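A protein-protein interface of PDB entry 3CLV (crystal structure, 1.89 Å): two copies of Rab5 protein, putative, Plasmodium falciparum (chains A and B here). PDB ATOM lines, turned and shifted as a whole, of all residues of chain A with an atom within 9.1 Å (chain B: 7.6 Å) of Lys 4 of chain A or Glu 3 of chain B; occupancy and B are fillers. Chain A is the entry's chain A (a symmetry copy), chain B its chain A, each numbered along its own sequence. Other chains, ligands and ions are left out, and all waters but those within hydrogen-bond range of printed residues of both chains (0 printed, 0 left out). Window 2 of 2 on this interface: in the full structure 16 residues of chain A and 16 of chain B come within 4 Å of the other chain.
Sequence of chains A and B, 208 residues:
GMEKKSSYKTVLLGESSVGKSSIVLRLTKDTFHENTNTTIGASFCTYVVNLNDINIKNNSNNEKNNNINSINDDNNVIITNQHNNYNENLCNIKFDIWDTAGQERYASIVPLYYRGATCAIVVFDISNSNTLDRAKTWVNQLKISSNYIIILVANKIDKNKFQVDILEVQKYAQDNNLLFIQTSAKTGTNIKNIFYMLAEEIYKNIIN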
ATOM      1  N   GLY A   1     -31.811  -6.400  15.496  1.00  0.00           N
ATOM      2  CA  GLY A   1     -30.329  -6.338  15.687  1.00  0.00           C
ATOM      3  C   GLY A   1     -29.795  -7.558  16.424  1.00  0.00           C
ATOM      4  O   GLY A   1     -30.556  -8.261  17.091  1.00  0.00           O
ATOM      5  N   MET A   2     -28.476  -7.762  16.370  1.00  0.00           N
ATOM      6  CA  MET A   2     -27.578  -6.688  15.964  1.00  0.00           C
ATOM      7  C   MET A   2     -26.685  -6.916  14.744  1.00  0.00           C
ATOM      8  O   MET A   2     -25.846  -7.818  14.711  1.00  0.00           O
ATOM      9  CB  MET A   2     -26.743  -6.210  17.165  1.00  0.00           C
ATOM     10  CG  MET A   2     -26.145  -4.828  16.981  1.00  0.00           C
ATOM     11  SD  MET A   2     -25.408  -4.188  18.498  1.00  0.00           S
ATOM     12  CE  MET A   2     -26.846  -3.868  19.514  1.00  0.00           C
ATOM     13  N   GLU A   3     -26.885  -6.039  13.764  1.00  0.00           N
ATOM     14  CA  GLU A   3     -25.992  -5.816  12.630  1.00  0.00           C
ATOM     15  C   GLU A   3     -24.590  -5.374  13.109  1.00  0.00           C
ATOM     16  O   GLU A   3     -24.477  -4.504  13.967  1.00  0.00           O
ATOM     17  CB  GLU A   3     -26.628  -4.724  11.750  1.00  0.00           C
ATOM     18  CG  GLU A   3     -25.746  -4.131  10.644  1.00  0.00           C
ATOM     19  CD  GLU A   3     -26.144  -2.691  10.246  1.00  0.00           C
ATOM     20  OE1 GLU A   3     -26.789  -1.963  11.053  1.00  0.00           O
ATOM     21  OE2 GLU A   3     -25.788  -2.277   9.119  1.00  0.00           O
ATOM     22  N   LYS A   4     -23.537  -5.985  12.563  1.00  0.00           N
ATOM     23  CA  LYS A   4     -22.156  -5.564  12.832  1.00  0.00           C
ATOM     24  C   LYS A   4     -21.848  -4.272  12.052  1.00  0.00           C
ATOM     25  O   LYS A   4     -22.202  -4.160  10.877  1.00  0.00           O
ATOM     26  CB  LYS A   4     -21.184  -6.697  12.457  1.00  0.00           C
ATOM     27  CG  LYS A   4     -19.704  -6.308  12.400  1.00  0.00           C
ATOM     28  CD  LYS A   4     -18.949  -7.117  11.345  1.00  0.00           C
ATOM     29  N   LYS A   5     -21.222  -3.289  12.708  1.00  0.00           N
ATOM     30  CA  LYS A   5     -20.940  -1.982  12.088  1.00  0.00           C
ATOM     31  C   LYS A   5     -19.463  -1.595  12.180  1.00  0.00           C
ATOM     32  O   LYS A   5     -18.760  -2.022  13.101  1.00  0.00           O
ATOM     33  CB  LYS A   5     -21.765  -0.868  12.739  1.00  0.00           C
ATOM     34  CG  LYS A   5     -23.235  -1.197  13.009  1.00  0.00           C
ATOM     35  CD  LYS A   5     -23.959  -0.010  13.650  1.00  0.00           C
ATOM     36  CE  LYS A   5     -24.130   1.118  12.659  1.00  0.00           C
ATOM     37  NZ  LYS A   5     -24.349   2.429  13.312  1.00  0.00           N
ATOM     38  N   SER A   6     -19.004  -0.761  11.246  1.00  0.00           N
ATOM     39  CA  SER A   6     -17.625  -0.253  11.284  1.00  0.00           C
ATOM     40  C   SER A   6     -17.380   0.683  12.472  1.00  0.00           C
ATOM     41  O   SER A   6     -16.253   0.805  12.941  1.00  0.00           O
ATOM     42  CB  SER A   6     -17.256   0.448   9.972  1.00  0.00           C
ATOM     43  OG  SER A   6     -18.195   1.473   9.698  1.00  0.00           O
ATOM     44  N   SER A   7     -18.429   1.370  12.924  1.00  0.00           N
ATOM     45  CA  SER A   7     -18.423   2.012  14.249  1.00  0.00           C
ATOM     46  C   SER A   7     -19.828   2.128  14.841  1.00  0.00           C
ATOM     47  O   SER A   7     -20.844   2.054  14.128  1.00  0.00           O
ATOM     48  CB  SER A   7     -17.705   3.370  14.249  1.00  0.00           C
ATOM     49  OG  SER A   7     -18.490   4.372  13.658  1.00  0.00           O
ATOM     50  N   TYR A   8     -19.868   2.318  16.151  1.00  0.00           N
ATOM     51  CA  TYR A   8     -21.106   2.321  16.898  1.00  0.00           C
ATOM     52  C   TYR A   8     -21.322   3.694  17.513  1.00  0.00           C
ATOM     53  O   TYR A   8     -20.608   4.089  18.454  1.00  0.00           O
ATOM     54  CB  TYR A   8     -21.082   1.211  17.951  1.00  0.00           C
ATOM     55  CG  TYR A   8     -20.908  -0.163  17.328  1.00  0.00           C
ATOM     56  CD1 TYR A   8     -22.006  -0.882  16.891  1.00  0.00           C
ATOM     57  CD2 TYR A   8     -19.637  -0.731  17.164  1.00  0.00           C
ATOM     58  CE1 TYR A   8     -21.869  -2.126  16.305  1.00  0.00           C
ATOM     59  CE2 TYR A   8     -19.485  -1.988  16.561  1.00  0.00           C
ATOM     60  CZ  TYR A   8     -20.615  -2.675  16.143  1.00  0.00           C
ATOM     61  OH  TYR A   8     -20.519  -3.913  15.548  1.00  0.00           O
ATOM     62  N   ASN A  87     -14.209 -13.738  18.246  1.00  0.00           N
ATOM     63  CA  ASN A  87     -14.007 -13.751  16.796  1.00  0.00           C
ATOM     64  C   ASN A  87     -13.357 -12.460  16.314  1.00  0.00           C
ATOM     65  O   ASN A  87     -13.944 -11.378  16.438  1.00  0.00           O
ATOM     66  CB  ASN A  87     -15.335 -13.984  16.060  1.00  0.00           C
ATOM     67  CG  ASN A  87     -15.863 -15.406  16.222  1.00  0.00           C
ATOM     68  OD1 ASN A  87     -15.341 -16.197  17.019  1.00  0.00           O
ATOM     69  ND2 ASN A  87     -16.902 -15.738  15.457  1.00  0.00           N
ATOM     70  N   GLU A  88     -12.154 -12.592  15.749  1.00  0.00           N
ATOM     71  CA  GLU A  88     -11.307 -11.455  15.348  1.00  0.00           C
ATOM     72  C   GLU A  88     -11.997 -10.436  14.439  1.00  0.00           C
ATOM     73  O   GLU A  88     -11.634  -9.255  14.429  1.00  0.00           O
ATOM     74  CB  GLU A  88     -10.009 -11.950  14.688  1.00  0.00           C
ATOM     75  CG  GLU A  88      -8.942 -12.483  15.666  1.00  0.00           C
ATOM     76  CD  GLU A  88      -9.203 -13.910  16.147  1.00  0.00           C
ATOM     77  OE1 GLU A  88     -10.022 -14.629  15.528  1.00  0.00           O
ATOM     78  OE2 GLU A  88      -8.580 -14.317  17.152  1.00  0.00           O
ATOM     79  N   ASN A  89     -12.992 -10.901  13.688  1.00  0.00           N
ATOM     80  CA  ASN A  89     -13.752 -10.049  12.772  1.00  0.00           C
ATOM     81  C   ASN A  89     -14.771  -9.149  13.479  1.00  0.00           C
ATOM     82  O   ASN A  89     -15.041  -8.030  13.028  1.00  0.00           O
ATOM     83  CB  ASN A  89     -14.458 -10.905  11.715  1.00  0.00           C
ATOM     84  CG  ASN A  89     -13.494 -11.787  10.942  1.00  0.00           C
ATOM     85  OD1 ASN A  89     -12.742 -11.309  10.089  1.00  0.00           O
ATOM     86  ND2 ASN A  89     -13.508 -13.084  11.241  1.00  0.00           N
ATOM     87  N   LEU A  90     -15.326  -9.642  14.585  1.00  0.00           N
ATOM     88  CA  LEU A  90     -16.425  -8.960  15.282  1.00  0.00           C
ATOM     89  C   LEU A  90     -15.983  -8.157  16.506  1.00  0.00           C
ATOM     90  O   LEU A  90     -16.679  -7.228  16.927  1.00  0.00           O
ATOM     91  CB  LEU A  90     -17.502  -9.974  15.706  1.00  0.00           C
ATOM     92  CG  LEU A  90     -18.098 -10.965  14.697  1.00  0.00           C
ATOM     93  CD1 LEU A  90     -19.095 -11.865  15.396  1.00  0.00           C
ATOM     94  CD2 LEU A  90     -18.754 -10.269  13.501  1.00  0.00           C
ATOM     95  N   CYS A  91     -14.824  -8.508  17.054  1.00  0.00           N
ATOM     96  CA  CYS A  91     -14.447  -8.099  18.404  1.00  0.00           C
ATOM     97  C   CYS A  91     -13.517  -6.890  18.470  1.00  0.00           C
ATOM     98  O   CYS A  91     -12.981  -6.564  19.543  1.00  0.00           O
ATOM     99  CB  CYS A  91     -13.801  -9.275  19.132  1.00  0.00           C
ATOM    100  SG  CYS A  91     -12.136  -9.589  18.543  1.00  0.00           S
ATOM    101  N   ASN A  92     -13.299  -6.249  17.329  1.00  0.00           N
ATOM    102  CA  ASN A  92     -12.654  -4.950  17.311  1.00  0.00           C
ATOM    103  C   ASN A  92     -13.754  -3.898  17.223  1.00  0.00           C
ATOM    104  O   ASN A  92     -14.313  -3.654  16.150  1.00  0.00           O
ATOM    105  CB  ASN A  92     -11.689  -4.843  16.136  1.00  0.00           C
ATOM    106  CG  ASN A  92     -10.762  -3.648  16.255  1.00  0.00           C
ATOM    107  OD1 ASN A  92      -9.850  -3.627  17.094  1.00  0.00           O
ATOM    108  ND2 ASN A  92     -10.978  -2.651  15.401  1.00  0.00           N
ATOM    109  N   ILE A  93     -14.074  -3.300  18.364  1.00  0.00           N
ATOM    110  CA  ILE A  93     -15.248  -2.438  18.467  1.00  0.00           C
ATOM    111  C   ILE A  93     -14.886  -0.963  18.587  1.00  0.00           C
ATOM    112  O   ILE A  93     -14.245  -0.536  19.556  1.00  0.00           O
ATOM    113  CB  ILE A  93     -16.178  -2.910  19.609  1.00  0.00           C
ATOM    114  CG1 ILE A  93     -16.748  -4.283  19.235  1.00  0.00           C
ATOM    115  CG2 ILE A  93     -17.303  -1.889  19.876  1.00  0.00           C
ATOM    116  CD1 ILE A  93     -16.907  -5.206  20.399  1.00  0.00           C
ATOM    117  N   THR A 118     -26.193   3.246  18.947  1.00  0.00           N
ATOM    118  CA  THR A 118     -26.180   1.869  19.461  1.00  0.00           C
ATOM    119  C   THR A 118     -26.159   1.908  20.977  1.00  0.00           C
ATOM    120  O   THR A 118     -26.853   1.142  21.637  1.00  0.00           O
ATOM    121  CB  THR A 118     -24.923   1.100  18.963  1.00  0.00           C
ATOM    122  OG1 THR A 118     -24.960   1.028  17.539  1.00  0.00           O
ATOM    123  CG2 THR A 118     -24.843  -0.325  19.555  1.00  0.00           C
ATOM    124  N   ILE A 202     -22.163  -5.183  23.061  1.00  0.00           N
ATOM    125  CA  ILE A 202     -22.347  -5.130  21.604  1.00  0.00           C
ATOM    126  C   ILE A 202     -22.028  -6.498  20.981  1.00  0.00           C
ATOM    127  O   ILE A 202     -22.784  -6.993  20.148  1.00  0.00           O
ATOM    128  CB  ILE A 202     -21.495  -4.029  20.918  1.00  0.00           C
ATOM    129  CG1 ILE A 202     -21.987  -2.634  21.316  1.00  0.00           C
ATOM    130  CG2 ILE A 202     -21.548  -4.173  19.394  1.00  0.00           C
ATOM    131  CD1 ILE A 202     -20.958  -1.507  20.993  1.00  0.00           C
ATOM    132  N   TYR A 203     -20.916  -7.099  21.406  1.00  0.00           N
ATOM    133  CA  TYR A 203     -20.464  -8.381  20.862  1.00  0.00           C
ATOM    134  C   TYR A 203     -21.490  -9.481  21.125  1.00  0.00           C
ATOM    135  O   TYR A 203     -21.859 -10.238  20.225  1.00  0.00           O
ATOM    136  CB  TYR A 203     -19.138  -8.785  21.504  1.00  0.00           C
ATOM    137  CG  TYR A 203     -18.554 -10.066  20.938  1.00  0.00           C
ATOM    138  CD1 TYR A 203     -17.885 -10.059  19.719  1.00  0.00           C
ATOM    139  CD2 TYR A 203     -18.680 -11.279  21.620  1.00  0.00           C
ATOM    140  CE1 TYR A 203     -17.339 -11.232  19.189  1.00  0.00           C
ATOM    141  CE2 TYR A 203     -18.142 -12.459  21.098  1.00  0.00           C
ATOM    142  CZ  TYR A 203     -17.474 -12.418  19.883  1.00  0.00           C
ATOM    143  OH  TYR A 203     -16.935 -13.565  19.340  1.00  0.00           O
ATOM    144  N   ASN A 205     -24.533  -9.123  21.531  1.00  0.00           N
ATOM    145  CA  ASN A 205     -25.640  -8.876  20.628  1.00  0.00           C
ATOM    146  C   ASN A 205     -25.417  -9.264  19.176  1.00  0.00           C
ATOM    147  O   ASN A 205     -26.307  -9.849  18.556  1.00  0.00           O
ATOM    148  CB  ASN A 205     -26.117  -7.426  20.735  1.00  0.00           C
ATOM    149  CG  ASN A 205     -27.073  -7.242  21.881  1.00  0.00           C
ATOM    150  OD1 ASN A 205     -28.266  -7.463  21.730  1.00  0.00           O
ATOM    151  ND2 ASN A 205     -26.548  -6.881  23.045  1.00  0.00           N
ATOM    152  N   ILE A 206     -24.250  -8.913  18.636  1.00  0.00           N
ATOM    153  CA  ILE A 206     -23.852  -9.292  17.272  1.00  0.00           C
ATOM    154  C   ILE A 206     -23.871 -10.813  17.167  1.00  0.00           C
ATOM    155  O   ILE A 206     -24.343 -11.360  16.177  1.00  0.00           O
ATOM    156  CB  ILE A 206     -22.415  -8.857  16.935  1.00  0.00           C
ATOM    157  CG1 ILE A 206     -22.263  -7.340  16.930  1.00  0.00           C
ATOM    158  CG2 ILE A 206     -21.983  -9.457  15.578  1.00  0.00           C
ATOM    159  CD1 ILE A 206     -20.794  -6.923  16.793  1.00  0.00           C
ATOM    160  N   ILE A 207     -23.314 -11.473  18.186  1.00  0.00           N
ATOM    161  CA  ILE A 207     -23.391 -12.927  18.332  1.00  0.00           C
ATOM    162  C   ILE A 207     -24.819 -13.370  18.674  1.00  0.00           C
ATOM    163  O   ILE A 207     -25.238 -14.473  18.310  1.00  0.00           O
ATOM    164  CB  ILE A 207     -22.376 -13.432  19.402  1.00  0.00           C
ATOM    165  CG1 ILE A 207     -20.962 -13.517  18.809  1.00  0.00           C
ATOM    166  CG2 ILE A 207     -22.805 -14.759  20.022  1.00  0.00           C
ATOM    167  CD1 ILE A 207     -20.828 -14.408  17.585  1.00  0.00           C
ATOM    168  N   GLY B   1     -14.474   2.330   2.362  1.00  0.00           N
ATOM    169  CA  GLY B   1     -15.872   1.906   2.041  1.00  0.00           C
ATOM    170  C   GLY B   1     -15.983   1.301   0.650  1.00  0.00           C
ATOM    171  O   GLY B   1     -15.109   1.518  -0.192  1.00  0.00           O
ATOM    172  N   MET B   2     -17.095   0.610   0.383  1.00  0.00           N
ATOM    173  CA  MET B   2     -18.275   0.755   1.225  1.00  0.00           C
ATOM    174  C   MET B   2     -18.826  -0.494   1.916  1.00  0.00           C
ATOM    175  O   MET B   2     -19.230  -1.467   1.277  1.00  0.00           O
ATOM    176  CB  MET B   2     -19.390   1.486   0.459  1.00  0.00           C
ATOM    177  CG  MET B   2     -20.450   2.096   1.356  1.00  0.00           C
ATOM    178  SD  MET B   2     -21.584   3.169   0.455  1.00  0.00           S
ATOM    179  CE  MET B   2     -20.546   4.571   0.055  1.00  0.00           C
ATOM    180  N   GLU B   3     -18.850  -0.403   3.243  1.00  0.00           N
ATOM    181  CA  GLU B   3     -19.590  -1.287   4.140  1.00  0.00           C
ATOM    182  C   GLU B   3     -21.104  -1.241   3.836  1.00  0.00           C
ATOM    183  O   GLU B   3     -21.670  -0.163   3.676  1.00  0.00           O
ATOM    184  CB  GLU B   3     -19.316  -0.817   5.580  1.00  0.00           C
ATOM    185  CG  GLU B   3     -20.195  -1.423   6.682  1.00  0.00           C
ATOM    186  CD  GLU B   3     -20.341  -0.513   7.923  1.00  0.00           C
ATOM    187  OE1 GLU B   3     -20.154   0.733   7.823  1.00  0.00           O
ATOM    188  OE2 GLU B   3     -20.669  -1.050   9.005  1.00  0.00           O
ATOM    189  N   LYS B   4     -21.746  -2.407   3.745  1.00  0.00           N
ATOM    190  CA  LYS B   4     -23.204  -2.495   3.595  1.00  0.00           C
ATOM    191  C   LYS B   4     -23.881  -2.195   4.946  1.00  0.00           C
ATOM    192  O   LYS B   4     -23.438  -2.692   5.983  1.00  0.00           O
ATOM    193  CB  LYS B   4     -23.591  -3.887   3.065  1.00  0.00           C
ATOM    194  CG  LYS B   4     -25.081  -4.233   3.138  1.00  0.00           C
ATOM    195  CD  LYS B   4     -25.302  -5.728   3.366  1.00  0.00           C
ATOM    196  N   LYS B   5     -24.928  -1.363   4.941  1.00  0.00           N
ATOM    197  CA  LYS B   5     -25.610  -0.946   6.180  1.00  0.00           C
ATOM    198  C   LYS B   5     -27.117  -1.202   6.135  1.00  0.00           C
ATOM    199  O   LYS B   5     -27.718  -1.213   5.056  1.00  0.00           O
ATOM    200  CB  LYS B   5     -25.388   0.543   6.462  1.00  0.00           C
ATOM    201  CG  LYS B   5     -23.961   1.056   6.258  1.00  0.00           C
ATOM    202  CD  LYS B   5     -23.858   2.549   6.578  1.00  0.00           C
ATOM    203  CE  LYS B   5     -24.005   2.795   8.062  1.00  0.00           C
ATOM    204  NZ  LYS B   5     -24.413   4.184   8.377  1.00  0.00           N
ATOM    205  N   SER B   6     -27.730  -1.372   7.307  1.00  0.00           N
ATOM    206  CA  SER B   6     -29.189  -1.538   7.391  1.00  0.00           C
ATOM    207  C   SER B   6     -29.945  -0.266   6.995  1.00  0.00           C
ATOM    208  O   SER B   6     -31.083  -0.339   6.544  1.00  0.00           O
ATOM    209  CB  SER B   6     -29.613  -1.994   8.791  1.00  0.00           C
ATOM    210  OG  SER B   6     -29.124  -1.083   9.760  1.00  0.00           O
ATOM    211  N   SER B   7     -29.325   0.895   7.205  1.00  0.00           N
ATOM    212  CA  SER B   7     -29.768   2.140   6.557  1.00  0.00           C
ATOM    213  C   SER B   7     -28.619   3.131   6.362  1.00  0.00           C
ATOM    214  O   SER B   7     -27.567   3.045   7.018  1.00  0.00           O
ATOM    215  CB  SER B   7     -30.953   2.798   7.281  1.00  0.00           C
ATOM    216  OG  SER B   7     -30.550   3.440   8.461  1.00  0.00           O
ATOM    217  N   TYR B   8     -28.842   4.072   5.458  1.00  0.00           N
ATOM    218  CA  TYR B   8     -27.823   5.013   5.050  1.00  0.00           C
ATOM    219  C   TYR B   8     -28.251   6.420   5.432  1.00  0.00           C
ATOM    220  O   TYR B   8     -29.188   6.984   4.834  1.00  0.00           O
ATOM    221  CB  TYR B   8     -27.557   4.875   3.549  1.00  0.00           C
ATOM    222  CG  TYR B   8     -27.089   3.478   3.178  1.00  0.00           C
ATOM    223  CD1 TYR B   8     -25.748   3.147   3.239  1.00  0.00           C
ATOM    224  CD2 TYR B   8     -27.998   2.488   2.784  1.00  0.00           C
ATOM    225  CE1 TYR B   8     -25.301   1.877   2.923  1.00  0.00           C
ATOM    226  CE2 TYR B   8     -27.559   1.193   2.471  1.00  0.00           C
ATOM    227  CZ  TYR B   8     -26.204   0.908   2.541  1.00  0.00           C
ATOM    228  OH  TYR B   8     -25.722  -0.348   2.241  1.00  0.00           O
ATOM    229  N   THR B 118     -23.849   8.890   4.723  1.00  0.00           N
ATOM    230  CA  THR B 118     -23.393   8.245   3.483  1.00  0.00           C
ATOM    231  C   THR B 118     -23.641   9.183   2.318  1.00  0.00           C
ATOM    232  O   THR B 118     -22.802   9.326   1.434  1.00  0.00           O
ATOM    233  CB  THR B 118     -24.164   6.918   3.230  1.00  0.00           C
ATOM    234  OG1 THR B 118     -23.902   6.019   4.306  1.00  0.00           O
ATOM    235  CG2 THR B 118     -23.761   6.261   1.891  1.00  0.00           C
ATOM    236  N   ILE B 202     -24.786   3.977  -4.176  1.00  0.00           N
ATOM    237  CA  ILE B 202     -24.434   3.201  -2.978  1.00  0.00           C
ATOM    238  C   ILE B 202     -24.101   1.753  -3.365  1.00  0.00           C
ATOM    239  O   ILE B 202     -23.102   1.202  -2.907  1.00  0.00           O
ATOM    240  CB  ILE B 202     -25.544   3.213  -1.893  1.00  0.00           C
ATOM    241  CG1 ILE B 202     -25.700   4.612  -1.289  1.00  0.00           C
ATOM    242  CG2 ILE B 202     -25.225   2.209  -0.781  1.00  0.00           C
ATOM    243  CD1 ILE B 202     -27.032   4.791  -0.498  1.00  0.00           C
ATOM    244  N   ASN B 205     -20.871   1.253  -5.035  1.00  0.00           N
ATOM    245  CA  ASN B 205     -19.834   1.310  -4.024  1.00  0.00           C
ATOM    246  C   ASN B 205     -19.681   0.074  -3.155  1.00  0.00           C
ATOM    247  O   ASN B 205     -18.555  -0.358  -2.899  1.00  0.00           O
ATOM    248  CB  ASN B 205     -19.984   2.565  -3.161  1.00  0.00           C
ATOM    249  CG  ASN B 205     -19.349   3.762  -3.811  1.00  0.00           C
ATOM    250  OD1 ASN B 205     -18.156   3.986  -3.660  1.00  0.00           O
ATOM    251  ND2 ASN B 205     -20.131   4.512  -4.577  1.00  0.00           N
ATOM    252  N   ILE B 206     -20.803  -0.469  -2.683  1.00  0.00           N
ATOM    253  CA  ILE B 206     -20.825  -1.714  -1.901  1.00  0.00           C
ATOM    254  C   ILE B 206     -20.196  -2.823  -2.739  1.00  0.00           C
ATOM    255  O   ILE B 206     -19.413  -3.617  -2.230  1.00  0.00           O
ATOM    256  CB  ILE B 206     -22.254  -2.181  -1.577  1.00  0.00           C
ATOM    257  CG1 ILE B 206     -22.987  -1.195  -0.673  1.00  0.00           C
ATOM    258  CG2 ILE B 206     -22.221  -3.589  -0.939  1.00  0.00           C
ATOM    259  CD1 ILE B 206     -24.467  -1.566  -0.520  1.00  0.00           C
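Glu 3 of chain A touches Lys 4 of chain B, and with the chains exchanged Lys 4 of chain A touches Glu 3 of chain B. Glu 3 of chain A touches Lys 5 of chain B, and with the chains exchanged Lys 5 of chain A touches Glu 3 of chain B. Glu 3 of chain A touches Ser 6 of chain B, and with the chains exchanged Ser 6 of chain A touches Glu 3 of chain B. Of the 6 pairs that touch across the chains among the printed residues, 6 have their exchanged pair printed and touching as well.
OH of Tyr 8 of chain A is in hydrogen-bond range of N of Lys 5 of chain A (3.0 Å). The backbone NH (N) of Lys 5 of chain B lies within hydrogen-bond range of the side-chain hydroxyl (OH) of Tyr 8 of chain B, at 3.0 Å.
OE2 of Glu 3 of chain B lies within hydrogen-bond range of N of Ser 6 of chain A (2.8 Å). The backbone NH (N) of Ser 6 of chain B is in hydrogen-bond range of the side-chain carboxylate (OE2) of Glu 3 of chain A.
Among the printed residues, merely in contact across the chains: Glu 3 of chain A with Lys 5 of chain B, Lys 5 of chain A with Glu 3 of chain B, Lys 4 of chain A with Glu 3 of chain B and Glu 3 of chain A with Lys 4 of chain B.
Printed residues of chain B within 4 Å of Glu 3 of chain A: Lys 4, Lys 5 and Ser 6. Of chain B, only Glu 3 comes within 4 Å of Lys 4 of chain A. Tyr 203 of chain A touches none of the printed residues of chain B. Of chain A, only Lys 4, Lys 5 and Ser 6 come within 4 Å of Glu 3 of chain B. Of the printed residues of chain A, Ser 6 of chain B touches Glu 3. The nearest residue of chain B that does not touch Lys 4 of chain A is Lys 4 of chain B (5.3 Å).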
